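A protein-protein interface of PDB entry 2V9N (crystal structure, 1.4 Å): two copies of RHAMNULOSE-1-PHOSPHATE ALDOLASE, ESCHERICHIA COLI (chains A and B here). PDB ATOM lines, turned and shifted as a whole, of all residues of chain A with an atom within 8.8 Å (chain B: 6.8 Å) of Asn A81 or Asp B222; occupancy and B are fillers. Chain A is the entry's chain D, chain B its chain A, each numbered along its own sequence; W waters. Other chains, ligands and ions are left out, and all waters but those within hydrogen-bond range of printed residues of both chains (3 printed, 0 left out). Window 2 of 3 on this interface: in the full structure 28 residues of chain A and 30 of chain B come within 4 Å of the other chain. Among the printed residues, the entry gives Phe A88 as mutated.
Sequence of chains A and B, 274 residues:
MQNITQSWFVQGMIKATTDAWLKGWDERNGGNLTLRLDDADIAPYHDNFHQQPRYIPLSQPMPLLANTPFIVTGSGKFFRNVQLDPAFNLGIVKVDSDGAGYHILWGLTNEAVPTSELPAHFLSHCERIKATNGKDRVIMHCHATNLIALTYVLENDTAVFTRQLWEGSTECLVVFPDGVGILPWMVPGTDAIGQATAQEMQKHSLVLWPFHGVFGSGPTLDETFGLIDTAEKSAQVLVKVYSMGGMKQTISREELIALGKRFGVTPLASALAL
Asn A81 touches two residues of chain B. Asp B222 touches just these residues of chain A: Phe A78 (3.2 Å) and Asn A81 (2.9 Å). Of the printed residues of chain A, Gly B226 touches Arg A28 (3.8 Å). Printed residues of chain B within 4 Å of Leu A84: Lys B15 (3.9 Å). Printed residues of chain B within 4 Å of Phe A78: Asp B222. Leu A90 touches none of the printed residues of chain B. The nearest residue of chain B that does not touch Asn A81 is Asp B19 (6.3 Å). The nearest printed residue of chain B that does not touch Phe A78 is Gly B226 (4.2 Å).
Among the printed residues, merely in contact across the chains: Phe A78 with Asp B222 (3.2 Å), Arg A80 with Lys B15 (3.6 Å), Arg A28 with Gly B226 (3.8 Å) and Leu A84 with Lys B15 (3.9 Å).
The side-chain amino group (NZ) of Lys B15 is in hydrogen-bond range of the side-chain amide oxygen (OD1) of Asn A81 (2.8 Å). NE of Arg A80 lies within salt-bridge range of OD2 of Asp B19 (2.8 Å). The side-chain carboxylate of Asp B222 lies within hydrogen-bond range of the side-chain amide nitrogen of Asn A81 (2.9 Å).
The side-chain carboxylate (OD2) of Asp B222 lies within salt-bridge range of the side-chain amino group (NZ) of Lys B15 (2.8 Å). The guanidinium group (NH1) of Arg A28 lies within hydrogen-bond range of the side-chain amide oxygen (OD1) of Asn A29, 3.0 Å away. The side-chain amide nitrogen (NE2) of Gln A83 sits close to the guanidinium group (NH1) of Arg A80 (3.2 Å). The backbone carbonyl oxygen (O) of Asn A81 lies within hydrogen-bond range of the side-chain amide nitrogen (ND2) of Asn A89, at 3.3 Å.
Of the 14 printed residues of chain B, 4 touch a printed residue of chain A. Printed residues of chain B that touch a printed residue of chain A: Lys B15, Asp B19, Asp B222 and Gly B226. Of the 23 printed residues of chain A, 5 touch a printed residue of chain B. Printed residues of chain A that touch a printed residue of chain B: Arg A28, Phe A78, Arg A80, Asn A81 and Leu A84. Hydrophobic or aromatic side chains of chain A that line the printed part of chain B: Phe A78 and Leu A84. Among the printed residues, Asp or Glu carboxylates within 4 Å of a Lys or Arg side-chain nitrogen of the other chain: Arg A80 with Asp B19.
Water W2 lies within hydrogen-bond range of the backbone carbonyl oxygen of Glu B223 (2.6 Å), the guanidinium group of Arg A28 (3.0 Å) and the backbone NH of Leu B227 (3.4 Å). Water W3 bridges OD1 of Asp B19 and NH2 of Arg A80. Water W1 bridges the side-chain carboxylate of Asp B19 (2.9 Å) and the indole nitrogen of Trp A21 (3.0 Å).
No position is printed for both chains.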
ATOM      1  N   ILE A  14      29.309  25.224  29.965  1.00  0.00           N
ATOM      2  CA  ILE A  14      28.663  23.937  29.715  1.00  0.00           C
ATOM      3  C   ILE A  14      27.769  23.556  30.908  1.00  0.00           C
ATOM      4  O   ILE A  14      26.604  23.173  30.741  1.00  0.00           O
ATOM      5  CB  ILE A  14      29.712  22.816  29.452  1.00  0.00           C
ATOM      6  CG1 ILE A  14      30.459  23.024  28.122  1.00  0.00           C
ATOM      7  CG2 ILE A  14      29.053  21.449  29.511  1.00  0.00           C
ATOM      8  CD1 ILE A  14      31.724  22.181  28.001  1.00  0.00           C
ATOM      9  N   THR A  17      24.493  25.959  31.149  1.00  0.00           N
ATOM     10  CA  THR A  17      23.531  25.717  30.078  1.00  0.00           C
ATOM     11  C   THR A  17      22.904  24.331  30.167  1.00  0.00           C
ATOM     12  O   THR A  17      21.704  24.152  29.886  1.00  0.00           O
ATOM     13  CB  THR A  17      24.160  25.915  28.684  1.00  0.00           C
ATOM     14  OG1 THR A  17      25.327  25.105  28.537  1.00  0.00           O
ATOM     15  CG2 THR A  17      24.512  27.377  28.467  1.00  0.00           C
ATOM     16  N   THR A  18      23.706  23.338  30.534  1.00  0.00           N
ATOM     17  CA  THR A  18      23.204  21.969  30.640  1.00  0.00           C
ATOM     18  C   THR A  18      22.221  21.867  31.814  1.00  0.00           C
ATOM     19  O   THR A  18      21.123  21.280  31.705  1.00  0.00           O
ATOM     20  CB  THR A  18      24.337  20.935  30.783  1.00  0.00           C
ATOM     21  OG1 THR A  18      25.268  21.067  29.692  1.00  0.00           O
ATOM     22  CG2 THR A  18      23.769  19.517  30.805  1.00  0.00           C
ATOM     23  N   TRP A  21      19.021  23.549  30.805  1.00  0.00           N
ATOM     24  CA  TRP A  21      18.304  22.610  29.927  1.00  0.00           C
ATOM     25  C   TRP A  21      17.535  21.559  30.760  1.00  0.00           C
ATOM     26  O   TRP A  21      16.357  21.342  30.526  1.00  0.00           O
ATOM     27  CB  TRP A  21      19.253  21.923  28.921  1.00  0.00           C
ATOM     28  CG  TRP A  21      18.670  20.639  28.355  1.00  0.00           C
ATOM     29  CD1 TRP A  21      19.048  19.354  28.650  1.00  0.00           C
ATOM     30  CD2 TRP A  21      17.556  20.537  27.474  1.00  0.00           C
ATOM     31  NE1 TRP A  21      18.238  18.460  27.979  1.00  0.00           N
ATOM     32  CE2 TRP A  21      17.311  19.166  27.260  1.00  0.00           C
ATOM     33  CE3 TRP A  21      16.746  21.477  26.832  1.00  0.00           C
ATOM     34  CZ2 TRP A  21      16.286  18.711  26.419  1.00  0.00           C
ATOM     35  CZ3 TRP A  21      15.728  21.032  25.999  1.00  0.00           C
ATOM     36  CH2 TRP A  21      15.509  19.660  25.791  1.00  0.00           C
ATOM     37  N   ASP A  26      14.843  25.948  28.841  1.00  0.00           N
ATOM     38  CA  ASP A  26      15.565  26.292  27.613  1.00  0.00           C
ATOM     39  C   ASP A  26      15.245  25.365  26.449  1.00  0.00           C
ATOM     40  O   ASP A  26      16.133  24.775  25.827  1.00  0.00           O
ATOM     41  CB  ASP A  26      17.051  26.337  27.926  1.00  0.00           C
ATOM     42  CG  ASP A  26      17.373  27.447  28.887  1.00  0.00           C
ATOM     43  OD1 ASP A  26      17.451  27.180  30.091  1.00  0.00           O
ATOM     44  OD2 ASP A  26      17.465  28.613  28.434  1.00  0.00           O
ATOM     45  N   GLU A  27      13.950  25.251  26.167  1.00  0.00           N
ATOM     46  CA  GLU A  27      13.465  24.576  24.982  1.00  0.00           C
ATOM     47  C   GLU A  27      14.061  25.214  23.736  1.00  0.00           C
ATOM     48  O   GLU A  27      14.263  26.425  23.723  1.00  0.00           O
ATOM     49  CB  GLU A  27      11.932  24.659  24.931  1.00  0.00           C
ATOM     50  CG  GLU A  27      11.337  26.055  24.631  1.00  0.00           C
ATOM     51  CD  GLU A  27      11.345  27.052  25.779  1.00  0.00           C
ATOM     52  OE1 GLU A  27      10.949  28.200  25.506  1.00  0.00           O
ATOM     53  OE2 GLU A  27      11.712  26.730  26.926  1.00  0.00           O
ATOM     54  N   ARG A  28      14.335  24.408  22.707  1.00  0.00           N
ATOM     55  CA  ARG A  28      14.851  24.907  21.424  1.00  0.00           C
ATOM     56  C   ARG A  28      16.075  25.796  21.710  1.00  0.00           C
ATOM     57  O   ARG A  28      16.966  25.365  22.441  1.00  0.00           O
ATOM     58  CB  ARG A  28      13.739  25.620  20.646  1.00  0.00           C
ATOM     59  CG  ARG A  28      13.987  25.803  19.140  1.00  0.00           C
ATOM     60  CD  ARG A  28      12.881  26.649  18.557  1.00  0.00           C
ATOM     61  NE  ARG A  28      12.911  26.797  17.093  1.00  0.00           N
ATOM     62  CZ  ARG A  28      13.325  27.884  16.437  1.00  0.00           C
ATOM     63  NH1 ARG A  28      13.831  28.922  17.079  1.00  0.00           N
ATOM     64  NH2 ARG A  28      13.253  27.920  15.110  1.00  0.00           N
ATOM     65  N   ASN A  29      16.109  27.019  21.179  1.00  0.00           N
ATOM     66  CA  ASN A  29      17.191  27.986  21.455  1.00  0.00           C
ATOM     67  C   ASN A  29      16.800  29.008  22.539  1.00  0.00           C
ATOM     68  O   ASN A  29      17.398  30.072  22.637  1.00  0.00           O
ATOM     69  CB  ASN A  29      17.527  28.735  20.175  1.00  0.00           C
ATOM     70  CG  ASN A  29      16.387  29.624  19.719  1.00  0.00           C
ATOM     71  OD1 ASN A  29      15.231  29.192  19.682  1.00  0.00           O
ATOM     72  ND2 ASN A  29      16.692  30.877  19.406  1.00  0.00           N
ATOM     73  N   GLY A  76      20.475  31.026  17.933  1.00  0.00           N
ATOM     74  CA  GLY A  76      19.780  29.839  17.433  1.00  0.00           C
ATOM     75  C   GLY A  76      20.307  28.518  17.972  1.00  0.00           C
ATOM     76  O   GLY A  76      19.783  27.460  17.622  1.00  0.00           O
ATOM     77  N   LYS A  77      21.335  28.575  18.818  1.00  0.00           N
ATOM     78  CA  LYS A  77      21.966  27.375  19.350  1.00  0.00           C
ATOM     79  C   LYS A  77      21.136  26.837  20.508  1.00  0.00           C
ATOM     80  O   LYS A  77      20.499  27.597  21.231  1.00  0.00           O
ATOM     81  CB  LYS A  77      23.395  27.674  19.808  1.00  0.00           C
ATOM     82  CG  LYS A  77      24.287  28.280  18.711  1.00  0.00           C
ATOM     83  CD  LYS A  77      24.514  27.346  17.530  1.00  0.00           C
ATOM     84  CE  LYS A  77      25.288  28.028  16.406  1.00  0.00           C
ATOM     85  NZ  LYS A  77      25.788  27.024  15.422  1.00  0.00           N
ATOM     86  N   PHE A  78      21.133  25.515  20.661  1.00  0.00           N
ATOM     87  CA  PHE A  78      20.361  24.844  21.716  1.00  0.00           C
ATOM     88  C   PHE A  78      21.224  24.678  22.976  1.00  0.00           C
ATOM     89  O   PHE A  78      22.309  24.096  22.906  1.00  0.00           O
ATOM     90  CB  PHE A  78      19.927  23.448  21.275  1.00  0.00           C
ATOM     91  CG  PHE A  78      18.784  23.405  20.263  1.00  0.00           C
ATOM     92  CD1 PHE A  78      18.403  24.502  19.492  1.00  0.00           C
ATOM     93  CD2 PHE A  78      18.090  22.215  20.084  1.00  0.00           C
ATOM     94  CE1 PHE A  78      17.336  24.396  18.575  1.00  0.00           C
ATOM     95  CE2 PHE A  78      17.075  22.103  19.173  1.00  0.00           C
ATOM     96  CZ  PHE A  78      16.692  23.189  18.419  1.00  0.00           C
ATOM     97  N   PHE A  79      20.748  25.155  24.128  1.00  0.00           N
ATOM     98  CA  PHE A  79      21.436  24.895  25.389  1.00  0.00           C
ATOM     99  C   PHE A  79      21.738  23.398  25.546  1.00  0.00           C
ATOM    100  O   PHE A  79      22.789  23.026  26.049  1.00  0.00           O
ATOM    101  CB  PHE A  79      20.591  25.361  26.588  1.00  0.00           C
ATOM    102  CG  PHE A  79      20.768  26.815  26.968  1.00  0.00           C
ATOM    103  CD1 PHE A  79      21.079  27.794  26.036  1.00  0.00           C
ATOM    104  CD2 PHE A  79      20.580  27.198  28.294  1.00  0.00           C
ATOM    105  CE1 PHE A  79      21.213  29.125  26.415  1.00  0.00           C
ATOM    106  CE2 PHE A  79      20.701  28.519  28.687  1.00  0.00           C
ATOM    107  CZ  PHE A  79      21.029  29.490  27.741  1.00  0.00           C
ATOM    108  N   ARG A  80      20.817  22.538  25.105  1.00  0.00           N
ATOM    109  CA  ARG A  80      20.992  21.080  25.201  1.00  0.00           C
ATOM    110  C   ARG A  80      22.260  20.568  24.520  1.00  0.00           C
ATOM    111  O   ARG A  80      22.809  19.537  24.931  1.00  0.00           O
ATOM    112  CB  ARG A  80      19.775  20.370  24.590  1.00  0.00           C
ATOM    113  CG  ARG A  80      19.708  18.861  24.859  1.00  0.00           C
ATOM    114  CD  ARG A  80      20.260  18.028  23.702  1.00  0.00           C
ATOM    115  NE  ARG A  80      20.248  16.622  24.039  1.00  0.00           N
ATOM    116  CZ  ARG A  80      21.191  15.983  24.718  1.00  0.00           C
ATOM    117  NH1 ARG A  80      22.320  16.581  25.069  1.00  0.00           N
ATOM    118  NH2 ARG A  80      21.002  14.714  25.005  1.00  0.00           N
ATOM    119  N   ASN A  81      22.700  21.257  23.470  1.00  0.00           N
ATOM    120  CA  ASN A  81      23.838  20.800  22.668  1.00  0.00           C
ATOM    121  C   ASN A  81      25.190  21.372  23.076  1.00  0.00           C
ATOM    122  O   ASN A  81      26.218  20.909  22.588  1.00  0.00           O
ATOM    123  CB  ASN A  81      23.611  21.148  21.198  1.00  0.00           C
ATOM    124  CG  ASN A  81      22.497  20.350  20.577  1.00  0.00           C
ATOM    125  OD1 ASN A  81      22.167  19.264  21.065  1.00  0.00           O
ATOM    126  ND2 ASN A  81      21.942  20.857  19.460  1.00  0.00           N
ATOM    127  N   VAL A  82      25.205  22.371  23.954  1.00  0.00           N
ATOM    128  CA  VAL A  82      26.466  23.005  24.351  1.00  0.00           C
ATOM    129  C   VAL A  82      27.484  21.960  24.830  1.00  0.00           C
ATOM    130  O   VAL A  82      28.662  22.000  24.448  1.00  0.00           O
ATOM    131  CB  VAL A  82      26.228  24.109  25.408  1.00  0.00           C
ATOM    132  CG1 VAL A  82      27.563  24.673  25.911  1.00  0.00           C
ATOM    133  CG2 VAL A  82      25.365  25.217  24.828  1.00  0.00           C
ATOM    134  N   GLN A  83      27.033  21.008  25.653  1.00  0.00           N
ATOM    135  CA  GLN A  83      27.907  19.956  26.156  1.00  0.00           C
ATOM    136  C   GLN A  83      28.484  19.068  25.053  1.00  0.00           C
ATOM    137  O   GLN A  83      29.543  18.451  25.244  1.00  0.00           O
ATOM    138  CB  GLN A  83      27.154  19.075  27.139  1.00  0.00           C
ATOM    139  CG  GLN A  83      26.004  18.279  26.517  1.00  0.00           C
ATOM    140  CD  GLN A  83      25.148  17.616  27.575  1.00  0.00           C
ATOM    141  OE1 GLN A  83      25.651  16.838  28.392  1.00  0.00           O
ATOM    142  NE2 GLN A  83      23.845  17.929  27.576  1.00  0.00           N
ATOM    143  N   LEU A  84      27.782  18.974  23.920  1.00  0.00           N
ATOM    144  CA  LEU A  84      28.178  18.076  22.823  1.00  0.00           C
ATOM    145  C   LEU A  84      29.207  18.705  21.881  1.00  0.00           C
ATOM    146  O   LEU A  84      30.029  17.993  21.275  1.00  0.00           O
ATOM    147  CB  LEU A  84      26.951  17.639  22.015  1.00  0.00           C
ATOM    148  CG  LEU A  84      25.847  16.971  22.829  1.00  0.00           C
ATOM    149  CD1 LEU A  84      24.687  16.585  21.915  1.00  0.00           C
ATOM    150  CD2 LEU A  84      26.373  15.748  23.564  1.00  0.00           C
ATOM    151  N   ASP A  85      29.173  20.025  21.760  1.00  0.00           N
ATOM    152  CA  ASP A  85      30.056  20.738  20.839  1.00  0.00           C
ATOM    153  C   ASP A  85      30.137  22.200  21.280  1.00  0.00           C
ATOM    154  O   ASP A  85      29.433  23.072  20.752  1.00  0.00           O
ATOM    155  CB  ASP A  85      29.554  20.594  19.401  1.00  0.00           C
ATOM    156  CG  ASP A  85      30.586  21.017  18.374  1.00  0.00           C
ATOM    157  OD1 ASP A  85      30.432  20.652  17.187  1.00  0.00           O
ATOM    158  OD2 ASP A  85      31.543  21.717  18.759  1.00  0.00           O
ATOM    159  N   PRO A  86      30.981  22.470  22.289  1.00  0.00           N
ATOM    160  CA  PRO A  86      31.139  23.830  22.806  1.00  0.00           C
ATOM    161  C   PRO A  86      31.493  24.862  21.732  1.00  0.00           C
ATOM    162  O   PRO A  86      30.907  25.941  21.707  1.00  0.00           O
ATOM    163  CB  PRO A  86      32.258  23.696  23.845  1.00  0.00           C
ATOM    164  CG  PRO A  86      32.342  22.269  24.160  1.00  0.00           C
ATOM    165  CD  PRO A  86      31.780  21.484  23.035  1.00  0.00           C
ATOM    166  N   ALA A  87      32.416  24.521  20.834  1.00  0.00           N
ATOM    167  CA  ALA A  87      32.856  25.466  19.797  1.00  0.00           C
ATOM    168  C   ALA A  87      31.757  25.825  18.782  1.00  0.00           C
ATOM    169  O   ALA A  87      31.772  26.916  18.213  1.00  0.00           O
ATOM    170  CB  ALA A  87      34.094  24.906  19.079  1.00  0.00           C
ATOM    171  N   PHE A  88      30.818  24.908  18.539  1.00  0.00           N
ATOM    172  CA  PHE A  88      29.703  25.157  17.615  1.00  0.00           C
ATOM    173  C   PHE A  88      28.621  26.042  18.252  1.00  0.00           C
ATOM    174  O   PHE A  88      27.894  26.763  17.565  1.00  0.00           O
ATOM    175  CB  PHE A  88      29.091  23.814  17.191  1.00  0.00           C
ATOM    176  CG  PHE A  88      28.019  23.925  16.135  1.00  0.00           C
ATOM    177  CD1 PHE A  88      28.356  24.167  14.809  1.00  0.00           C
ATOM    178  CD2 PHE A  88      26.679  23.746  16.454  1.00  0.00           C
ATOM    179  CE1 PHE A  88      27.373  24.254  13.825  1.00  0.00           C
ATOM    180  CE2 PHE A  88      25.696  23.838  15.473  1.00  0.00           C
ATOM    181  CZ  PHE A  88      26.045  24.088  14.161  1.00  0.00           C
ATOM    182  N   ASN A  89      28.511  25.966  19.577  1.00  0.00           N
ATOM    183  CA  ASN A  89      27.403  26.580  20.302  1.00  0.00           C
ATOM    184  C   ASN A  89      27.759  27.816  21.127  1.00  0.00           C
ATOM    185  O   ASN A  89      26.867  28.569  21.526  1.00  0.00           O
ATOM    186  CB  ASN A  89      26.756  25.510  21.189  1.00  0.00           C
ATOM    187  CG  ASN A  89      26.048  24.470  20.373  1.00  0.00           C
ATOM    188  OD1 ASN A  89      25.011  24.761  19.781  1.00  0.00           O
ATOM    189  ND2 ASN A  89      26.621  23.271  20.284  1.00  0.00           N
ATOM    190  N   LEU A  90      29.054  27.994  21.398  1.00  0.00           N
ATOM    191  CA  LEU A  90      29.554  29.101  22.192  1.00  0.00           C
ATOM    192  C   LEU A  90      30.605  29.837  21.401  1.00  0.00           C
ATOM    193  O   LEU A  90      31.178  29.293  20.461  1.00  0.00           O
ATOM    194  CB  LEU A  90      30.224  28.602  23.474  1.00  0.00           C
ATOM    195  CG  LEU A  90      29.431  27.711  24.410  1.00  0.00           C
ATOM    196  CD1 LEU A  90      30.324  27.291  25.591  1.00  0.00           C
ATOM    197  CD2 LEU A  90      28.161  28.406  24.893  1.00  0.00           C
ATOM    198  N   GLY B  12      21.966  10.431  16.215  1.00  0.00           N
ATOM    199  CA  GLY B  12      20.898  11.435  16.237  1.00  0.00           C
ATOM    200  C   GLY B  12      19.557  10.854  16.649  1.00  0.00           C
ATOM    201  O   GLY B  12      18.832  11.462  17.434  1.00  0.00           O
ATOM    202  N   LYS B  15      19.653  10.205  20.311  1.00  0.00           N
ATOM    203  CA  LYS B  15      19.518  11.418  21.120  1.00  0.00           C
ATOM    204  C   LYS B  15      18.060  11.895  21.199  1.00  0.00           C
ATOM    205  O   LYS B  15      17.578  12.246  22.269  1.00  0.00           O
ATOM    206  CB  LYS B  15      20.411  12.551  20.596  1.00  0.00           C
ATOM    207  CG  LYS B  15      20.561  13.716  21.584  1.00  0.00           C
ATOM    208  CD  LYS B  15      21.319  14.910  21.007  1.00  0.00           C
ATOM    209  CE  LYS B  15      20.395  15.915  20.376  1.00  0.00           C
ATOM    210  NZ  LYS B  15      21.118  17.026  19.691  1.00  0.00           N
ATOM    211  N   ALA B  16      17.374  11.930  20.059  1.00  0.00           N
ATOM    212  CA  ALA B  16      16.020  12.456  20.023  1.00  0.00           C
ATOM    213  C   ALA B  16      15.056  11.556  20.798  1.00  0.00           C
ATOM    214  O   ALA B  16      14.244  12.040  21.581  1.00  0.00           O
ATOM    215  CB  ALA B  16      15.542  12.640  18.570  1.00  0.00           C
ATOM    216  N   ASP B  19      15.914  11.763  24.590  1.00  0.00           N
ATOM    217  CA  ASP B  19      15.484  13.043  25.159  1.00  0.00           C
ATOM    218  C   ASP B  19      13.957  13.075  25.305  1.00  0.00           C
ATOM    219  O   ASP B  19      13.433  13.576  26.308  1.00  0.00           O
ATOM    220  CB  ASP B  19      15.924  14.220  24.295  1.00  0.00           C
ATOM    221  CG  ASP B  19      17.417  14.499  24.341  1.00  0.00           C
ATOM    222  OD1 ASP B  19      18.137  13.977  25.214  1.00  0.00           O
ATOM    223  OD2 ASP B  19      17.846  15.282  23.470  1.00  0.00           O
ATOM    224  N   VAL B 138      12.335  15.228   8.464  1.00  0.00           N
ATOM    225  CA  VAL B 138      11.979  14.530   9.697  1.00  0.00           C
ATOM    226  C   VAL B 138      10.490  14.662   9.986  1.00  0.00           C
ATOM    227  O   VAL B 138       9.935  15.755   9.866  1.00  0.00           O
ATOM    228  CB  VAL B 138      12.755  15.110  10.915  1.00  0.00           C
ATOM    229  CG1 VAL B 138      12.299  14.426  12.214  1.00  0.00           C
ATOM    230  CG2 VAL B 138      14.273  14.967  10.729  1.00  0.00           C
ATOM    231  N   PRO B 219      13.592  20.242   9.090  1.00  0.00           N
ATOM    232  CA  PRO B 219      14.763  19.862   8.294  1.00  0.00           C
ATOM    233  C   PRO B 219      15.758  18.918   8.965  1.00  0.00           C
ATOM    234  O   PRO B 219      16.463  18.185   8.277  1.00  0.00           O
ATOM    235  CB  PRO B 219      15.443  21.214   7.981  1.00  0.00           C
ATOM    236  CG  PRO B 219      14.467  22.265   8.387  1.00  0.00           C
ATOM    237  CD  PRO B 219      13.632  21.661   9.472  1.00  0.00           C
ATOM    238  N   THR B 220      15.822  18.966  10.295  1.00  0.00           N
ATOM    239  CA  THR B 220      16.737  18.151  11.074  1.00  0.00           C
ATOM    240  C   THR B 220      16.028  17.609  12.299  1.00  0.00           C
ATOM    241  O   THR B 220      14.960  18.109  12.694  1.00  0.00           O
ATOM    242  CB  THR B 220      17.962  18.947  11.533  1.00  0.00           C
ATOM    243  OG1 THR B 220      17.554  19.952  12.469  1.00  0.00           O
ATOM    244  CG2 THR B 220      18.649  19.592  10.342  1.00  0.00           C
ATOM    245  N   LEU B 221      16.616  16.584  12.898  1.00  0.00           N
ATOM    246  CA  LEU B 221      16.100  16.055  14.153  1.00  0.00           C
ATOM    247  C   LEU B 221      15.963  17.150  15.214  1.00  0.00           C
ATOM    248  O   LEU B 221      14.909  17.276  15.852  1.00  0.00           O
ATOM    249  CB  LEU B 221      16.974  14.911  14.657  1.00  0.00           C
ATOM    250  CG  LEU B 221      16.880  13.610  13.845  1.00  0.00           C
ATOM    251  CD1 LEU B 221      18.002  12.635  14.229  1.00  0.00           C
ATOM    252  CD2 LEU B 221      15.510  12.960  14.027  1.00  0.00           C
ATOM    253  N   ASP B 222      17.020  17.937  15.421  1.00  0.00           N
ATOM    254  CA  ASP B 222      16.982  18.981  16.451  1.00  0.00           C
ATOM    255  C   ASP B 222      15.920  20.036  16.176  1.00  0.00           C
ATOM    256  O   ASP B 222      15.215  20.463  17.091  1.00  0.00           O
ATOM    257  CB  ASP B 222      18.346  19.672  16.601  1.00  0.00           C
ATOM    258  CG  ASP B 222      19.296  18.926  17.517  1.00  0.00           C
ATOM    259  OD1 ASP B 222      20.502  19.247  17.473  1.00  0.00           O
ATOM    260  OD2 ASP B 222      18.853  18.052  18.307  1.00  0.00           O
ATOM    261  N   GLU B 223      15.791  20.472  14.929  1.00  0.00           N
ATOM    262  CA  GLU B 223      14.810  21.516  14.646  1.00  0.00           C
ATOM    263  C   GLU B 223      13.374  21.023  14.844  1.00  0.00           C
ATOM    264  O   GLU B 223      12.512  21.786  15.273  1.00  0.00           O
ATOM    265  CB  GLU B 223      14.999  22.067  13.235  1.00  0.00           C
ATOM    266  CG  GLU B 223      16.286  22.819  13.051  1.00  0.00           C
ATOM    267  CD  GLU B 223      16.564  23.108  11.597  1.00  0.00           C
ATOM    268  OE1 GLU B 223      15.972  24.075  11.083  1.00  0.00           O
ATOM    269  OE2 GLU B 223      17.354  22.368  10.972  1.00  0.00           O
ATOM    270  N   THR B 224      13.132  19.747  14.557  1.00  0.00           N
ATOM    271  CA  THR B 224      11.794  19.153  14.697  1.00  0.00           C
ATOM    272  C   THR B 224      11.498  18.899  16.170  1.00  0.00           C
ATOM    273  O   THR B 224      10.413  19.209  16.641  1.00  0.00           O
ATOM    274  CB  THR B 224      11.657  17.832  13.887  1.00  0.00           C
ATOM    275  OG1 THR B 224      12.137  18.043  12.554  1.00  0.00           O
ATOM    276  CG2 THR B 224      10.212  17.348  13.842  1.00  0.00           C
ATOM    277  N   PHE B 225      12.468  18.337  16.892  1.00  0.00           N
ATOM    278  CA  PHE B 225      12.356  18.173  18.338  1.00  0.00           C
ATOM    279  C   PHE B 225      12.092  19.527  19.013  1.00  0.00           C
ATOM    280  O   PHE B 225      11.187  19.648  19.831  1.00  0.00           O
ATOM    281  CB  PHE B 225      13.624  17.540  18.915  1.00  0.00           C
ATOM    282  CG  PHE B 225      13.508  17.187  20.366  1.00  0.00           C
ATOM    283  CD1 PHE B 225      13.243  15.887  20.769  1.00  0.00           C
ATOM    284  CD2 PHE B 225      13.622  18.170  21.336  1.00  0.00           C
ATOM    285  CE1 PHE B 225      13.112  15.576  22.101  1.00  0.00           C
ATOM    286  CE2 PHE B 225      13.480  17.857  22.676  1.00  0.00           C
ATOM    287  CZ  PHE B 225      13.242  16.554  23.053  1.00  0.00           C
ATOM    288  N   GLY B 226      12.885  20.536  18.658  1.00  0.00           N
ATOM    289  CA  GLY B 226      12.747  21.881  19.221  1.00  0.00           C
ATOM    290  C   GLY B 226      11.420  22.544  18.938  1.00  0.00           C
ATOM    291  O   GLY B 226      10.911  23.294  19.757  1.00  0.00           O
ATOM    292  N   LEU B 227      10.870  22.275  17.761  1.00  0.00           N
ATOM    293  CA  LEU B 227       9.539  22.760  17.371  1.00  0.00           C
ATOM    294  C   LEU B 227       8.458  22.223  18.317  1.00  0.00           C
ATOM    295  O   LEU B 227       7.651  22.970  18.883  1.00  0.00           O
ATOM    296  CB  LEU B 227       9.262  22.339  15.921  1.00  0.00           C
ATOM    297  CG  LEU B 227       7.854  22.559  15.363  1.00  0.00           C
ATOM    298  CD1 LEU B 227       7.540  24.044  15.239  1.00  0.00           C
ATOM    299  CD2 LEU B 227       7.715  21.839  14.018  1.00  0.00           C
HETATM  300  O   HOH W   1      17.905  15.514  27.637  1.00  0.00           O
HETATM  301  O   HOH W   2      12.183  24.390  15.442  1.00  0.00           O
HETATM  302  O   HOH W   3      19.625  11.842  26.089  1.00  0.00           O
